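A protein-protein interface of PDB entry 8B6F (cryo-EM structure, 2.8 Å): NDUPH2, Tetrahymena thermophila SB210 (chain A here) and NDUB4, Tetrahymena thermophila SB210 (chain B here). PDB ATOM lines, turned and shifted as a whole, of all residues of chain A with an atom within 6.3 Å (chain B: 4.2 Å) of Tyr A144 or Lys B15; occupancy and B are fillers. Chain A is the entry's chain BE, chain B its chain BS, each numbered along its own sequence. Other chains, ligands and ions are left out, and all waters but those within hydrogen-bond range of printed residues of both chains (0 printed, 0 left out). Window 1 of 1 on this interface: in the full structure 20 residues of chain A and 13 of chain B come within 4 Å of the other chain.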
ATOM      1  N   LEU A 115     -13.960 -31.703   7.571  1.00  0.00           N
ATOM      2  CA  LEU A 115     -14.159 -30.282   7.823  1.00  0.00           C
ATOM      3  C   LEU A 115     -14.464 -30.060   9.298  1.00  0.00           C
ATOM      4  O   LEU A 115     -15.383 -30.677   9.845  1.00  0.00           O
ATOM      5  CB  LEU A 115     -15.291 -29.733   6.950  1.00  0.00           C
ATOM      6  CG  LEU A 115     -15.516 -28.218   6.921  1.00  0.00           C
ATOM      7  CD1 LEU A 115     -16.300 -27.826   5.686  1.00  0.00           C
ATOM      8  CD2 LEU A 115     -16.248 -27.718   8.153  1.00  0.00           C
ATOM      9  N   ILE A 116     -13.695 -29.177   9.932  1.00  0.00           N
ATOM     10  CA  ILE A 116     -13.924 -28.823  11.334  1.00  0.00           C
ATOM     11  C   ILE A 116     -13.784 -27.322  11.500  1.00  0.00           C
ATOM     12  O   ILE A 116     -13.076 -26.651  10.736  1.00  0.00           O
ATOM     13  CB  ILE A 116     -12.940 -29.542  12.280  1.00  0.00           C
ATOM     14  CG1 ILE A 116     -11.501 -29.089  12.002  1.00  0.00           C
ATOM     15  CG2 ILE A 116     -13.068 -31.046  12.109  1.00  0.00           C
ATOM     16  CD1 ILE A 116     -10.458 -29.732  12.895  1.00  0.00           C
ATOM     17  N   PRO A 117     -14.457 -26.762  12.501  1.00  0.00           N
ATOM     18  CA  PRO A 117     -14.319 -25.329  12.770  1.00  0.00           C
ATOM     19  C   PRO A 117     -13.065 -25.015  13.567  1.00  0.00           C
ATOM     20  O   PRO A 117     -12.573 -25.830  14.351  1.00  0.00           O
ATOM     21  CB  PRO A 117     -15.580 -25.004  13.576  1.00  0.00           C
ATOM     22  CG  PRO A 117     -15.869 -26.260  14.304  1.00  0.00           C
ATOM     23  CD  PRO A 117     -15.435 -27.392  13.406  1.00  0.00           C
ATOM     24  N   VAL A 118     -12.546 -23.809  13.353  1.00  0.00           N
ATOM     25  CA  VAL A 118     -11.378 -23.338  14.099  1.00  0.00           C
ATOM     26  C   VAL A 118     -11.575 -21.881  14.478  1.00  0.00           C
ATOM     27  O   VAL A 118     -12.257 -21.117  13.784  1.00  0.00           O
ATOM     28  CB  VAL A 118     -10.074 -23.486  13.287  1.00  0.00           C
ATOM     29  CG1 VAL A 118      -9.750 -24.953  13.067  1.00  0.00           C
ATOM     30  CG2 VAL A 118     -10.182 -22.757  11.957  1.00  0.00           C
ATOM     31  N   PRO A 119     -10.985 -21.469  15.599  1.00  0.00           N
ATOM     32  CA  PRO A 119     -11.010 -20.050  15.966  1.00  0.00           C
ATOM     33  C   PRO A 119     -10.158 -19.206  15.031  1.00  0.00           C
ATOM     34  O   PRO A 119      -9.225 -19.682  14.384  1.00  0.00           O
ATOM     35  CB  PRO A 119     -10.441 -20.036  17.390  1.00  0.00           C
ATOM     36  CG  PRO A 119     -10.621 -21.409  17.892  1.00  0.00           C
ATOM     37  CD  PRO A 119     -10.488 -22.305  16.708  1.00  0.00           C
ATOM     38  N   THR A 140     -14.136 -13.301  10.476  1.00  0.00           N
ATOM     39  CA  THR A 140     -13.270 -14.026  11.398  1.00  0.00           C
ATOM     40  C   THR A 140     -14.009 -15.140  12.127  1.00  0.00           C
ATOM     41  O   THR A 140     -13.416 -16.187  12.406  1.00  0.00           O
ATOM     42  CB  THR A 140     -12.656 -13.058  12.411  1.00  0.00           C
ATOM     43  OG1 THR A 140     -13.697 -12.409  13.153  1.00  0.00           O
ATOM     44  CG2 THR A 140     -11.817 -12.007  11.702  1.00  0.00           C
ATOM     45  N   GLU A 141     -15.288 -14.938  12.449  1.00  0.00           N
ATOM     46  CA  GLU A 141     -16.034 -15.958  13.176  1.00  0.00           C
ATOM     47  C   GLU A 141     -16.182 -17.229  12.352  1.00  0.00           C
ATOM     48  O   GLU A 141     -16.028 -18.338  12.876  1.00  0.00           O
ATOM     49  CB  GLU A 141     -17.413 -15.432  13.578  1.00  0.00           C
ATOM     50  CG  GLU A 141     -17.389 -14.266  14.555  1.00  0.00           C
ATOM     51  CD  GLU A 141     -17.180 -12.926  13.877  1.00  0.00           C
ATOM     52  OE1 GLU A 141     -17.067 -12.892  12.634  1.00  0.00           O
ATOM     53  OE2 GLU A 141     -17.130 -11.902  14.590  1.00  0.00           O
ATOM     54  N   MET A 142     -16.485 -17.091  11.063  1.00  0.00           N
ATOM     55  CA  MET A 142     -16.766 -18.237  10.200  1.00  0.00           C
ATOM     56  C   MET A 142     -15.493 -18.609   9.447  1.00  0.00           C
ATOM     57  O   MET A 142     -15.333 -18.342   8.257  1.00  0.00           O
ATOM     58  CB  MET A 142     -17.912 -17.915   9.245  1.00  0.00           C
ATOM     59  CG  MET A 142     -19.165 -17.400   9.938  1.00  0.00           C
ATOM     60  SD  MET A 142     -19.861 -18.573  11.115  1.00  0.00           S
ATOM     61  CE  MET A 142     -20.419 -19.872  10.018  1.00  0.00           C
ATOM     62  N   ILE A 143     -14.571 -19.241  10.168  1.00  0.00           N
ATOM     63  CA  ILE A 143     -13.351 -19.797   9.597  1.00  0.00           C
ATOM     64  C   ILE A 143     -13.344 -21.289   9.890  1.00  0.00           C
ATOM     65  O   ILE A 143     -13.511 -21.697  11.044  1.00  0.00           O
ATOM     66  CB  ILE A 143     -12.090 -19.117  10.165  1.00  0.00           C
ATOM     67  CG1 ILE A 143     -12.039 -17.652   9.723  1.00  0.00           C
ATOM     68  CG2 ILE A 143     -10.832 -19.855   9.715  1.00  0.00           C
ATOM     69  CD1 ILE A 143     -10.929 -16.846  10.369  1.00  0.00           C
ATOM     70  N   TYR A 144     -13.156 -22.097   8.853  1.00  0.00           N
ATOM     71  CA  TYR A 144     -13.189 -23.544   8.984  1.00  0.00           C
ATOM     72  C   TYR A 144     -11.854 -24.128   8.538  1.00  0.00           C
ATOM     73  O   TYR A 144     -11.041 -23.464   7.891  1.00  0.00           O
ATOM     74  CB  TYR A 144     -14.347 -24.139   8.179  1.00  0.00           C
ATOM     75  CG  TYR A 144     -15.692 -23.848   8.802  1.00  0.00           C
ATOM     76  CD1 TYR A 144     -16.366 -22.666   8.524  1.00  0.00           C
ATOM     77  CD2 TYR A 144     -16.274 -24.738   9.692  1.00  0.00           C
ATOM     78  CE1 TYR A 144     -17.591 -22.391   9.099  1.00  0.00           C
ATOM     79  CE2 TYR A 144     -17.497 -24.473  10.271  1.00  0.00           C
ATOM     80  CZ  TYR A 144     -18.147 -23.297   9.973  1.00  0.00           C
ATOM     81  OH  TYR A 144     -19.365 -23.034  10.549  1.00  0.00           O
ATOM     82  N   PHE A 145     -11.636 -25.392   8.893  1.00  0.00           N
ATOM     83  CA  PHE A 145     -10.358 -26.060   8.677  1.00  0.00           C
ATOM     84  C   PHE A 145     -10.598 -27.443   8.093  1.00  0.00           C
ATOM     85  O   PHE A 145     -11.314 -28.254   8.685  1.00  0.00           O
ATOM     86  CB  PHE A 145      -9.567 -26.157   9.986  1.00  0.00           C
ATOM     87  CG  PHE A 145      -8.212 -26.780   9.830  1.00  0.00           C
ATOM     88  CD1 PHE A 145      -7.167 -26.057   9.286  1.00  0.00           C
ATOM     89  CD2 PHE A 145      -7.978 -28.076  10.250  1.00  0.00           C
ATOM     90  CE1 PHE A 145      -5.916 -26.620   9.146  1.00  0.00           C
ATOM     91  CE2 PHE A 145      -6.727 -28.647  10.112  1.00  0.00           C
ATOM     92  CZ  PHE A 145      -5.696 -27.916   9.561  1.00  0.00           C
ATOM     93  N   ASN A 146     -10.003 -27.703   6.933  1.00  0.00           N
ATOM     94  CA  ASN A 146      -9.974 -29.040   6.358  1.00  0.00           C
ATOM     95  C   ASN A 146      -8.733 -29.759   6.873  1.00  0.00           C
ATOM     96  O   ASN A 146      -7.606 -29.337   6.599  1.00  0.00           O
ATOM     97  CB  ASN A 146      -9.964 -28.977   4.832  1.00  0.00           C
ATOM     98  CG  ASN A 146      -9.981 -30.351   4.189  1.00  0.00           C
ATOM     99  OD1 ASN A 146      -9.801 -31.366   4.859  1.00  0.00           O
ATOM    100  ND2 ASN A 146     -10.192 -30.390   2.881  1.00  0.00           N
ATOM    101  N   GLU A 151      -5.773 -27.211   5.603  1.00  0.00           N
ATOM    102  CA  GLU A 151      -6.057 -25.950   4.938  1.00  0.00           C
ATOM    103  C   GLU A 151      -7.168 -25.221   5.681  1.00  0.00           C
ATOM    104  O   GLU A 151      -7.947 -25.824   6.422  1.00  0.00           O
ATOM    105  CB  GLU A 151      -6.446 -26.183   3.474  1.00  0.00           C
ATOM    106  CG  GLU A 151      -6.488 -24.933   2.626  1.00  0.00           C
ATOM    107  CD  GLU A 151      -6.695 -25.249   1.163  1.00  0.00           C
ATOM    108  OE1 GLU A 151      -6.967 -26.425   0.845  1.00  0.00           O
ATOM    109  OE2 GLU A 151      -6.580 -24.328   0.329  1.00  0.00           O
ATOM    110  N   PHE A 152      -7.237 -23.911   5.465  1.00  0.00           N
ATOM    111  CA  PHE A 152      -8.250 -23.055   6.066  1.00  0.00           C
ATOM    112  C   PHE A 152      -9.179 -22.501   4.997  1.00  0.00           C
ATOM    113  O   PHE A 152      -8.752 -22.218   3.873  1.00  0.00           O
ATOM    114  CB  PHE A 152      -7.609 -21.897   6.834  1.00  0.00           C
ATOM    115  CG  PHE A 152      -6.802 -22.331   8.018  1.00  0.00           C
ATOM    116  CD1 PHE A 152      -5.467 -22.658   7.878  1.00  0.00           C
ATOM    117  CD2 PHE A 152      -7.380 -22.414   9.273  1.00  0.00           C
ATOM    118  CE1 PHE A 152      -4.723 -23.060   8.965  1.00  0.00           C
ATOM    119  CE2 PHE A 152      -6.641 -22.816  10.366  1.00  0.00           C
ATOM    120  CZ  PHE A 152      -5.310 -23.139  10.212  1.00  0.00           C
ATOM    121  N   TYR A 153     -10.452 -22.353   5.353  1.00  0.00           N
ATOM    122  CA  TYR A 153     -11.455 -21.729   4.499  1.00  0.00           C
ATOM    123  C   TYR A 153     -11.988 -20.493   5.206  1.00  0.00           C
ATOM    124  O   TYR A 153     -12.466 -20.582   6.341  1.00  0.00           O
ATOM    125  CB  TYR A 153     -12.594 -22.697   4.180  1.00  0.00           C
ATOM    126  CG  TYR A 153     -12.141 -23.965   3.502  1.00  0.00           C
ATOM    127  CD1 TYR A 153     -11.417 -23.919   2.320  1.00  0.00           C
ATOM    128  CD2 TYR A 153     -12.452 -25.205   4.034  1.00  0.00           C
ATOM    129  CE1 TYR A 153     -11.005 -25.072   1.692  1.00  0.00           C
ATOM    130  CE2 TYR A 153     -12.045 -26.365   3.415  1.00  0.00           C
ATOM    131  CZ  TYR A 153     -11.323 -26.292   2.243  1.00  0.00           C
ATOM    132  OH  TYR A 153     -10.918 -27.449   1.623  1.00  0.00           O
ATOM    133  N   VAL A 154     -11.916 -19.350   4.531  1.00  0.00           N
ATOM    134  CA  VAL A 154     -12.348 -18.072   5.083  1.00  0.00           C
ATOM    135  C   VAL A 154     -13.444 -17.519   4.185  1.00  0.00           C
ATOM    136  O   VAL A 154     -13.268 -17.431   2.965  1.00  0.00           O
ATOM    137  CB  VAL A 154     -11.178 -17.077   5.192  1.00  0.00           C
ATOM    138  CG1 VAL A 154     -11.638 -15.779   5.839  1.00  0.00           C
ATOM    139  CG2 VAL A 154     -10.024 -17.691   5.971  1.00  0.00           C
ATOM    140  N   PHE A 155     -14.565 -17.147   4.788  1.00  0.00           N
ATOM    141  CA  PHE A 155     -15.713 -16.620   4.067  1.00  0.00           C
ATOM    142  C   PHE A 155     -15.741 -15.098   4.148  1.00  0.00           C
ATOM    143  O   PHE A 155     -14.958 -14.469   4.863  1.00  0.00           O
ATOM    144  CB  PHE A 155     -17.010 -17.210   4.627  1.00  0.00           C
ATOM    145  CG  PHE A 155     -17.096 -18.702   4.504  1.00  0.00           C
ATOM    146  CD1 PHE A 155     -16.559 -19.524   5.481  1.00  0.00           C
ATOM    147  CD2 PHE A 155     -17.710 -19.284   3.410  1.00  0.00           C
ATOM    148  CE1 PHE A 155     -16.636 -20.896   5.370  1.00  0.00           C
ATOM    149  CE2 PHE A 155     -17.790 -20.656   3.293  1.00  0.00           C
ATOM    150  CZ  PHE A 155     -17.252 -21.463   4.275  1.00  0.00           C
ATOM    151  N   TRP A 161     -26.437 -16.369   3.444  1.00  0.00           N
ATOM    152  CA  TRP A 161     -26.463 -17.768   3.849  1.00  0.00           C
ATOM    153  C   TRP A 161     -27.863 -18.330   3.654  1.00  0.00           C
ATOM    154  O   TRP A 161     -28.851 -17.690   4.024  1.00  0.00           O
ATOM    155  CB  TRP A 161     -26.033 -17.925   5.308  1.00  0.00           C
ATOM    156  CG  TRP A 161     -24.598 -17.600   5.554  1.00  0.00           C
ATOM    157  CD1 TRP A 161     -24.060 -16.362   5.749  1.00  0.00           C
ATOM    158  CD2 TRP A 161     -23.511 -18.528   5.638  1.00  0.00           C
ATOM    159  NE1 TRP A 161     -22.704 -16.462   5.946  1.00  0.00           N
ATOM    160  CE2 TRP A 161     -22.342 -17.781   5.883  1.00  0.00           C
ATOM    161  CE3 TRP A 161     -23.413 -19.919   5.527  1.00  0.00           C
ATOM    162  CZ2 TRP A 161     -21.091 -18.378   6.020  1.00  0.00           C
ATOM    163  CZ3 TRP A 161     -22.170 -20.511   5.662  1.00  0.00           C
ATOM    164  CH2 TRP A 161     -21.025 -19.740   5.906  1.00  0.00           C
ATOM    165  N   PHE B  10     -22.164 -24.209  10.481  1.00  0.00           N
ATOM    166  CA  PHE B  10     -22.396 -22.996   9.701  1.00  0.00           C
ATOM    167  C   PHE B  10     -23.403 -22.091  10.395  1.00  0.00           C
ATOM    168  O   PHE B  10     -23.809 -21.074   9.817  1.00  0.00           O
ATOM    169  CB  PHE B  10     -22.873 -23.287   8.275  1.00  0.00           C
ATOM    170  CG  PHE B  10     -21.988 -24.241   7.526  1.00  0.00           C
ATOM    171  CD1 PHE B  10     -20.617 -24.229   7.718  1.00  0.00           C
ATOM    172  CD2 PHE B  10     -22.529 -25.154   6.638  1.00  0.00           C
ATOM    173  CE1 PHE B  10     -19.800 -25.105   7.033  1.00  0.00           C
ATOM    174  CE2 PHE B  10     -21.716 -26.035   5.949  1.00  0.00           C
ATOM    175  CZ  PHE B  10     -20.350 -26.009   6.147  1.00  0.00           C
ATOM    176  N   SER B  11     -23.823 -22.427  11.613  1.00  0.00           N
ATOM    177  CA  SER B  11     -24.644 -21.530  12.410  1.00  0.00           C
ATOM    178  C   SER B  11     -23.746 -20.551  13.152  1.00  0.00           C
ATOM    179  O   SER B  11     -22.791 -20.958  13.821  1.00  0.00           O
ATOM    180  CB  SER B  11     -25.496 -22.326  13.398  1.00  0.00           C
ATOM    181  OG  SER B  11     -26.293 -21.467  14.193  1.00  0.00           O
ATOM    182  N   ARG B  12     -24.051 -19.257  13.035  1.00  0.00           N
ATOM    183  CA  ARG B  12     -23.165 -18.242  13.595  1.00  0.00           C
ATOM    184  C   ARG B  12     -23.074 -18.359  15.110  1.00  0.00           C
ATOM    185  O   ARG B  12     -21.988 -18.229  15.686  1.00  0.00           O
ATOM    186  CB  ARG B  12     -23.643 -16.850  13.187  1.00  0.00           C
ATOM    187  CG  ARG B  12     -22.706 -15.731  13.609  1.00  0.00           C
ATOM    188  CD  ARG B  12     -22.981 -14.460  12.827  1.00  0.00           C
ATOM    189  NE  ARG B  12     -22.677 -14.617  11.409  1.00  0.00           N
ATOM    190  CZ  ARG B  12     -21.477 -14.441  10.872  1.00  0.00           C
ATOM    191  NH1 ARG B  12     -20.433 -14.096  11.607  1.00  0.00           N
ATOM    192  NH2 ARG B  12     -21.321 -14.617   9.563  1.00  0.00           N
ATOM    193  N   GLN B  13     -24.204 -18.599  15.777  1.00  0.00           N
ATOM    194  CA  GLN B  13     -24.193 -18.692  17.234  1.00  0.00           C
ATOM    195  C   GLN B  13     -23.348 -19.870  17.697  1.00  0.00           C
ATOM    196  O   GLN B  13     -22.524 -19.738  18.609  1.00  0.00           O
ATOM    197  CB  GLN B  13     -25.622 -18.810  17.769  1.00  0.00           C
ATOM    198  CG  GLN B  13     -26.503 -17.597  17.486  1.00  0.00           C
ATOM    199  CD  GLN B  13     -27.068 -17.590  16.077  1.00  0.00           C
ATOM    200  OE1 GLN B  13     -26.900 -18.546  15.322  1.00  0.00           O
ATOM    201  NE2 GLN B  13     -27.744 -16.504  15.717  1.00  0.00           N
ATOM    202  N   PHE B  14     -23.544 -21.038  17.083  1.00  0.00           N
ATOM    203  CA  PHE B  14     -22.767 -22.212  17.465  1.00  0.00           C
ATOM    204  C   PHE B  14     -21.288 -22.022  17.157  1.00  0.00           C
ATOM    205  O   PHE B  14     -20.425 -22.443  17.935  1.00  0.00           O
ATOM    206  CB  PHE B  14     -23.305 -23.452  16.755  1.00  0.00           C
ATOM    207  CG  PHE B  14     -22.538 -24.701  17.062  1.00  0.00           C
ATOM    208  CD1 PHE B  14     -22.816 -25.435  18.203  1.00  0.00           C
ATOM    209  CD2 PHE B  14     -21.538 -25.142  16.212  1.00  0.00           C
ATOM    210  CE1 PHE B  14     -22.112 -26.587  18.490  1.00  0.00           C
ATOM    211  CE2 PHE B  14     -20.828 -26.293  16.493  1.00  0.00           C
ATOM    212  CZ  PHE B  14     -21.116 -27.016  17.634  1.00  0.00           C
ATOM    213  N   LYS B  15     -20.975 -21.392  16.024  1.00  0.00           N
ATOM    214  CA  LYS B  15     -19.577 -21.147  15.683  1.00  0.00           C
ATOM    215  C   LYS B  15     -18.917 -20.225  16.698  1.00  0.00           C
ATOM    216  O   LYS B  15     -17.782 -20.468  17.122  1.00  0.00           O
ATOM    217  CB  LYS B  15     -19.471 -20.558  14.276  1.00  0.00           C
ATOM    218  CG  LYS B  15     -19.153 -21.582  13.193  1.00  0.00           C
ATOM    219  CD  LYS B  15     -17.755 -22.186  13.344  1.00  0.00           C
ATOM    220  CE  LYS B  15     -16.659 -21.147  13.156  1.00  0.00           C
ATOM    221  NZ  LYS B  15     -15.302 -21.759  13.185  1.00  0.00           N
ATOM    222  N   LYS B  16     -19.612 -19.163  17.107  1.00  0.00           N
ATOM    223  CA  LYS B  16     -19.061 -18.283  18.131  1.00  0.00           C
ATOM    224  C   LYS B  16     -18.871 -19.030  19.443  1.00  0.00           C
ATOM    225  O   LYS B  16     -17.852 -18.858  20.122  1.00  0.00           O
ATOM    226  CB  LYS B  16     -19.969 -17.070  18.331  1.00  0.00           C
ATOM    227  CG  LYS B  16     -19.909 -16.058  17.198  1.00  0.00           C
ATOM    228  CD  LYS B  16     -20.787 -14.852  17.492  1.00  0.00           C
ATOM    229  CE  LYS B  16     -20.587 -13.756  16.457  1.00  0.00           C
ATOM    230  NZ  LYS B  16     -21.494 -12.597  16.687  1.00  0.00           N
ATOM    231  N   ALA B  17     -19.841 -19.863  19.819  1.00  0.00           N
ATOM    232  CA  ALA B  17     -19.717 -20.630  21.053  1.00  0.00           C
ATOM    233  C   ALA B  17     -18.498 -21.541  21.007  1.00  0.00           C
ATOM    234  O   ALA B  17     -17.731 -21.621  21.973  1.00  0.00           O
ATOM    235  CB  ALA B  17     -20.988 -21.444  21.293  1.00  0.00           C
ATOM    236  N   PHE B  18     -18.304 -22.243  19.888  1.00  0.00           N
ATOM    237  CA  PHE B  18     -17.150 -23.129  19.766  1.00  0.00           C
ATOM    238  C   PHE B  18     -15.844 -22.346  19.770  1.00  0.00           C
ATOM    239  O   PHE B  18     -14.864 -22.771  20.392  1.00  0.00           O
ATOM    240  CB  PHE B  18     -17.256 -23.971  18.497  1.00  0.00           C
ATOM    241  CG  PHE B  18     -16.116 -24.932  18.322  1.00  0.00           C
ATOM    242  CD1 PHE B  18     -16.149 -26.181  18.919  1.00  0.00           C
ATOM    243  CD2 PHE B  18     -15.005 -24.583  17.573  1.00  0.00           C
ATOM    244  CE1 PHE B  18     -15.100 -27.065  18.767  1.00  0.00           C
ATOM    245  CE2 PHE B  18     -13.952 -25.462  17.418  1.00  0.00           C
ATOM    246  CZ  PHE B  18     -14.000 -26.705  18.015  1.00  0.00           C
ATOM    247  N   ASN B  19     -15.805 -21.203  19.083  1.00  0.00           N
ATOM    248  CA  ASN B  19     -14.585 -20.403  19.067  1.00  0.00           C
ATOM    249  C   ASN B  19     -14.205 -19.953  20.469  1.00  0.00           C
ATOM    250  O   ASN B  19     -13.024 -19.965  20.835  1.00  0.00           O
ATOM    251  CB  ASN B  19     -14.765 -19.189  18.154  1.00  0.00           C
ATOM    252  CG  ASN B  19     -14.974 -19.572  16.707  1.00  0.00           C
ATOM    253  OD1 ASN B  19     -14.545 -20.637  16.266  1.00  0.00           O
ATOM    254  ND2 ASN B  19     -15.629 -18.699  15.953  1.00  0.00           N
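O of Ile A143 sits at hydrogen-bond distance from NZ of Lys B15, 2.8 Å away. The guanidinium group (NH1) of Arg B12 lies within salt-bridge range of the side-chain carboxylate (OE1) of Glu A141 (3.7 Å). O of Glu A141 sits at hydrogen-bond distance from ND2 of Asn B19 (3.1 Å). The side-chain amide oxygen (OD1) of Asn B19 sits close to the backbone carbonyl oxygen (O) of Val A118. N of Phe B10 sits at hydrogen-bond distance from OH of Tyr A144 (3.0 Å). O of Val A118 sits at hydrogen-bond distance from NZ of Lys B15, 3.2 Å away.
The backbone NH of Val A118 sits at hydrogen-bond distance from the backbone carbonyl oxygen of Ile A143, 3.3 Å away. The backbone carbonyl oxygen (O) of Tyr A144 is in hydrogen-bond range of the backbone NH (N) of Tyr A153, 2.8 Å away. ND2 of Asn B19 lies close to O of Lys B15, at 3.0 Å. OG1 of Thr A140 is in hydrogen-bond range of OE1 of Glu A141.
Among the printed residues, pairs that only touch across the chains: Glu A141 with Lys B15 (2.9 Å), Tyr A144 with Lys B15 (3.0 Å), Pro A117 with Lys B15 (3.3 Å), Pro A117 with Phe B18 (3.4 Å), Met A142 with Arg B12 (3.5 Å), Pro A119 with Asn B19 (3.6 Å), Met A142 with Phe B10 (3.6 Å), Met A142 with Lys B15 (3.7 Å), Glu A141 with Lys B16 (3.8 Å) and Trp A161 with Phe B10 (3.9 Å).
Of the printed residues of chain B, Val A118 touches Lys B15 and Asn B19. Tyr A144 touches just these residues of chain B: Phe B10 (3.0 Å) and Lys B15 (3.0 Å). Lys B15 touches just these residues of chain A: Pro A117 (3.3 Å), Val A118 (3.2 Å), Glu A141 (2.9 Å), Met A142 (3.7 Å), Ile A143 (2.8 Å) and Tyr A144 (3.0 Å). Printed residues of chain A within 4 Å of Phe B18: Pro A117. Printed residues of chain A within 4 Å of Asn B19: Val A118 (3.4 Å), Pro A119 (3.6 Å) and Glu A141 (3.1 Å).
Of the 10 printed residues of chain B, 6 touch a printed residue of chain A. Printed residues of chain B that touch a printed residue of chain A: Phe B10, Arg B12, Lys B15, Lys B16, Phe B18 and Asn B19. Among the printed residues, Asp or Glu carboxylates within 4 Å of a Lys or Arg side-chain nitrogen of the other chain: Glu A141 with Arg B12 (3.7 Å).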
